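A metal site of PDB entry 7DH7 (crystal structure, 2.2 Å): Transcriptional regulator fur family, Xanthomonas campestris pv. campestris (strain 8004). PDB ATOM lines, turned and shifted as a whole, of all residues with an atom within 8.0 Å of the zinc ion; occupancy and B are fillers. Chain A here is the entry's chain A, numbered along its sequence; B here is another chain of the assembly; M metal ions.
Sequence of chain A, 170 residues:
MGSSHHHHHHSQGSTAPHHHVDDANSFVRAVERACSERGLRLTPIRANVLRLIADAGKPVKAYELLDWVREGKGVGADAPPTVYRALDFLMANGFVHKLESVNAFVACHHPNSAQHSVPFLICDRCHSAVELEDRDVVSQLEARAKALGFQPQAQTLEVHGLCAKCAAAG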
ATOM      1  N   GLU A 100     -20.818   2.895   4.301  1.00  0.00           N
ATOM      2  CA  GLU A 100     -21.909   1.964   4.557  1.00  0.00           C
ATOM      3  C   GLU A 100     -21.408   0.559   4.852  1.00  0.00           C
ATOM      4  O   GLU A 100     -22.159  -0.243   5.441  1.00  0.00           O
ATOM      5  CB  GLU A 100     -22.868   1.920   3.381  1.00  0.00           C
ATOM      6  CG  GLU A 100     -24.258   2.361   3.776  1.00  0.00           C
ATOM      7  CD  GLU A 100     -25.059   2.899   2.617  1.00  0.00           C
ATOM      8  OE1 GLU A 100     -25.338   2.116   1.679  1.00  0.00           O
ATOM      9  OE2 GLU A 100     -25.415   4.093   2.647  1.00  0.00           O
ATOM     10  N   ILE A 122     -17.287   7.714  -3.924  1.00  0.00           N
ATOM     11  CA  ILE A 122     -18.392   8.382  -3.245  1.00  0.00           C
ATOM     12  C   ILE A 122     -19.476   8.757  -4.251  1.00  0.00           C
ATOM     13  O   ILE A 122     -19.178   9.254  -5.349  1.00  0.00           O
ATOM     14  CB  ILE A 122     -17.899   9.642  -2.498  1.00  0.00           C
ATOM     15  CG1 ILE A 122     -16.711   9.305  -1.592  1.00  0.00           C
ATOM     16  CG2 ILE A 122     -19.015  10.316  -1.696  1.00  0.00           C
ATOM     17  CD1 ILE A 122     -15.464  10.023  -2.039  1.00  0.00           C
ATOM     18  N   CYS A 123     -20.732   8.549  -3.860  1.00  0.00           N
ATOM     19  CA  CYS A 123     -21.858   8.948  -4.693  1.00  0.00           C
ATOM     20  C   CYS A 123     -22.270  10.407  -4.451  1.00  0.00           C
ATOM     21  O   CYS A 123     -22.473  10.824  -3.305  1.00  0.00           O
ATOM     22  CB  CYS A 123     -23.042   8.016  -4.459  1.00  0.00           C
ATOM     23  SG  CYS A 123     -24.523   8.454  -5.364  1.00  0.00           S
ATOM     24  N   ASP A 124     -22.465  11.124  -5.570  1.00  0.00           N
ATOM     25  CA  ASP A 124     -22.836  12.546  -5.591  1.00  0.00           C
ATOM     26  C   ASP A 124     -24.140  12.831  -4.878  1.00  0.00           C
ATOM     27  O   ASP A 124     -24.373  13.955  -4.409  1.00  0.00           O
ATOM     28  CB  ASP A 124     -23.021  13.037  -7.028  1.00  0.00           C
ATOM     29  CG  ASP A 124     -21.793  13.554  -7.623  1.00  0.00           C
ATOM     30  OD1 ASP A 124     -20.819  13.701  -6.853  1.00  0.00           O
ATOM     31  OD2 ASP A 124     -21.781  13.784  -8.862  1.00  0.00           O
ATOM     32  N   ARG A 125     -25.088  11.900  -4.953  1.00  0.00           N
ATOM     33  CA  ARG A 125     -26.463  12.166  -4.569  1.00  0.00           C
ATOM     34  C   ARG A 125     -26.727  11.753  -3.143  1.00  0.00           C
ATOM     35  O   ARG A 125     -27.399  12.466  -2.387  1.00  0.00           O
ATOM     36  CB  ARG A 125     -27.435  11.399  -5.474  1.00  0.00           C
ATOM     37  CG  ARG A 125     -27.413  11.865  -6.892  1.00  0.00           C
ATOM     38  CD  ARG A 125     -27.931  13.294  -6.985  1.00  0.00           C
ATOM     39  NE  ARG A 125     -29.232  13.445  -6.323  1.00  0.00           N
ATOM     40  CZ  ARG A 125     -30.380  13.028  -6.851  1.00  0.00           C
ATOM     41  NH1 ARG A 125     -30.384  12.430  -8.030  1.00  0.00           N
ATOM     42  NH2 ARG A 125     -31.526  13.223  -6.203  1.00  0.00           N
ATOM     43  N   CYS A 126     -26.194  10.597  -2.775  1.00  0.00           N
ATOM     44  CA  CYS A 126     -26.461   9.969  -1.494  1.00  0.00           C
ATOM     45  C   CYS A 126     -25.297  10.028  -0.503  1.00  0.00           C
ATOM     46  O   CYS A 126     -25.519   9.816   0.687  1.00  0.00           O
ATOM     47  CB  CYS A 126     -26.932   8.535  -1.770  1.00  0.00           C
ATOM     48  SG  CYS A 126     -25.719   7.245  -1.758  1.00  0.00           S
ATOM     49  N   HIS A 127     -24.075  10.353  -0.950  1.00  0.00           N
ATOM     50  CA  HIS A 127     -22.917  10.578  -0.090  1.00  0.00           C
ATOM     51  C   HIS A 127     -22.459   9.322   0.638  1.00  0.00           C
ATOM     52  O   HIS A 127     -21.788   9.408   1.684  1.00  0.00           O
ATOM     53  CB  HIS A 127     -23.168  11.716   0.914  1.00  0.00           C
ATOM     54  CG  HIS A 127     -23.982  12.835   0.330  1.00  0.00           C
ATOM     55  ND1 HIS A 127     -23.566  13.544  -0.776  1.00  0.00           N
ATOM     56  CD2 HIS A 127     -25.200  13.334   0.667  1.00  0.00           C
ATOM     57  CE1 HIS A 127     -24.482  14.446  -1.094  1.00  0.00           C
ATOM     58  NE2 HIS A 127     -25.486  14.322  -0.239  1.00  0.00           N
ATOM     59  N   SER A 128     -22.812   8.155   0.125  1.00  0.00           N
ATOM     60  CA  SER A 128     -22.191   6.933   0.604  1.00  0.00           C
ATOM     61  C   SER A 128     -20.825   6.754  -0.036  1.00  0.00           C
ATOM     62  O   SER A 128     -20.594   7.159  -1.179  1.00  0.00           O
ATOM     63  CB  SER A 128     -23.071   5.720   0.300  1.00  0.00           C
ATOM     64  OG  SER A 128     -24.323   5.889   0.943  1.00  0.00           O
ATOM     65  N   ALA A 129     -19.902   6.185   0.719  1.00  0.00           N
ATOM     66  CA  ALA A 129     -18.550   5.927   0.243  1.00  0.00           C
ATOM     67  C   ALA A 129     -18.243   4.450   0.345  1.00  0.00           C
ATOM     68  O   ALA A 129     -18.674   3.774   1.280  1.00  0.00           O
ATOM     69  CB  ALA A 129     -17.529   6.717   1.056  1.00  0.00           C
ATOM     70  N   GLY A 161     -18.831   9.729  -8.188  1.00  0.00           N
ATOM     71  CA  GLY A 161     -19.683   9.217  -9.233  1.00  0.00           C
ATOM     72  C   GLY A 161     -21.102   9.112  -8.750  1.00  0.00           C
ATOM     73  O   GLY A 161     -21.496   9.811  -7.808  1.00  0.00           O
ATOM     74  N   LEU A 162     -21.854   8.213  -9.343  1.00  0.00           N
ATOM     75  CA  LEU A 162     -23.261   8.003  -8.970  1.00  0.00           C
ATOM     76  C   LEU A 162     -23.466   6.529  -8.631  1.00  0.00           C
ATOM     77  O   LEU A 162     -23.051   5.727  -9.427  1.00  0.00           O
ATOM     78  CB  LEU A 162     -24.106   8.444 -10.165  1.00  0.00           C
ATOM     79  CG  LEU A 162     -25.615   8.512  -9.962  1.00  0.00           C
ATOM     80  CD1 LEU A 162     -25.973   9.531  -8.891  1.00  0.00           C
ATOM     81  CD2 LEU A 162     -26.285   8.888 -11.270  1.00  0.00           C
ATOM     82  N   CYS A 163     -24.096   6.213  -7.495  1.00  0.00           N
ATOM     83  CA  CYS A 163     -24.375   4.800  -7.102  1.00  0.00           C
ATOM     84  C   CYS A 163     -25.456   4.209  -8.017  1.00  0.00           C
ATOM     85  O   CYS A 163     -26.243   4.948  -8.586  1.00  0.00           O
ATOM     86  CB  CYS A 163     -24.852   4.690  -5.656  1.00  0.00           C
ATOM     87  SG  CYS A 163     -26.482   5.403  -5.376  1.00  0.00           S
ATOM     88  N   ALA A 164     -25.494   2.895  -8.110  1.00  0.00           N
ATOM     89  CA  ALA A 164     -26.518   2.244  -8.944  1.00  0.00           C
ATOM     90  C   ALA A 164     -27.924   2.571  -8.418  1.00  0.00           C
ATOM     91  O   ALA A 164     -28.797   2.819  -9.216  1.00  0.00           O
ATOM     92  CB  ALA A 164     -26.266   0.763  -8.982  1.00  0.00           C
ATOM     93  N   LYS A 165     -28.108   2.593  -7.099  1.00  0.00           N
ATOM     94  CA  LYS A 165     -29.429   2.888  -6.501  1.00  0.00           C
ATOM     95  C   LYS A 165     -29.887   4.323  -6.796  1.00  0.00           C
ATOM     96  O   LYS A 165     -31.055   4.465  -7.071  1.00  0.00           O
ATOM     97  CB  LYS A 165     -29.432   2.646  -4.992  1.00  0.00           C
ATOM     98  CG  LYS A 165     -28.678   1.417  -4.533  1.00  0.00           C
ATOM     99  CD  LYS A 165     -29.284   0.800  -3.319  1.00  0.00           C
ATOM    100  CE  LYS A 165     -28.315  -0.055  -2.552  1.00  0.00           C
ATOM    101  NZ  LYS A 165     -28.979  -0.778  -1.443  1.00  0.00           N
ATOM    102  N   CYS A 166     -29.027   5.329  -6.669  1.00  0.00           N
ATOM    103  CA  CYS A 166     -29.494   6.707  -6.991  1.00  0.00           C
ATOM    104  C   CYS A 166     -29.703   6.857  -8.492  1.00  0.00           C
ATOM    105  O   CYS A 166     -30.559   7.624  -8.866  1.00  0.00           O
ATOM    106  CB  CYS A 166     -28.717   7.847  -6.333  1.00  0.00           C
ATOM    107  SG  CYS A 166     -28.724   7.717  -4.530  1.00  0.00           S
ATOM    108  N   ALA A 167     -28.914   6.129  -9.296  1.00  0.00           N
ATOM    109  CA  ALA A 167     -29.020   6.156 -10.776  1.00  0.00           C
ATOM    110  C   ALA A 167     -30.383   5.638 -11.242  1.00  0.00           C
ATOM    111  O   ALA A 167     -30.870   6.136 -12.234  1.00  0.00           O
ATOM    112  CB  ALA A 167     -27.878   5.428 -11.434  1.00  0.00           C
ATOM    113  N   GLY B 149     -20.610  -1.214  -6.999  1.00  0.00           N
ATOM    114  CA  GLY B 149     -21.982  -0.720  -6.885  1.00  0.00           C
ATOM    115  C   GLY B 149     -22.287   0.604  -7.559  1.00  0.00           C
ATOM    116  O   GLY B 149     -23.399   1.059  -7.396  1.00  0.00           O
ATOM    117  N   PHE B 150     -21.367   1.147  -8.349  1.00  0.00           N
ATOM    118  CA  PHE B 150     -21.598   2.437  -8.990  1.00  0.00           C
ATOM    119  C   PHE B 150     -21.860   2.281 -10.487  1.00  0.00           C
ATOM    120  O   PHE B 150     -21.589   1.238 -11.082  1.00  0.00           O
ATOM    121  CB  PHE B 150     -20.401   3.376  -8.753  1.00  0.00           C
ATOM    122  CG  PHE B 150     -20.357   3.975  -7.351  1.00  0.00           C
ATOM    123  CD1 PHE B 150     -20.197   3.176  -6.241  1.00  0.00           C
ATOM    124  CD2 PHE B 150     -20.504   5.341  -7.172  1.00  0.00           C
ATOM    125  CE1 PHE B 150     -20.177   3.732  -4.961  1.00  0.00           C
ATOM    126  CE2 PHE B 150     -20.484   5.897  -5.891  1.00  0.00           C
ATOM    127  CZ  PHE B 150     -20.310   5.081  -4.789  1.00  0.00           C
HETATM  128 ZN    ZN M   1     -26.127   7.075  -4.115  1.00  0.00          ZN
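The zinc ion is bound by the side-chain sulfur of Cys 163, the side-chain sulfur of Cys 126, the side-chain sulfur of Cys 123 and the side-chain sulfur of Cys 166. The zinc ion has four donor atoms within binding distance.
The backbone NH (N) of Lys 165 lies close to the side-chain sulfur (SG) of Cys 163, at 3.7 Å. SG of Cys 126 sits close to OG of Ser 128 (3.3 Å). N of Arg 125 sits close to SG of Cys 123, 3.5 Å away. N of Cys 123 is in hydrogen-bond range of O of Ser 128, at 3.0 Å.
Of the 18 residues printed, 4 come within 4 Å of the zinc ion. Along chain A the residues within 4 Å of the zinc ion span positions 123 to 166. The nearest printed residue that does not touch the zinc ion is Arg 125 (4.7 Å).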
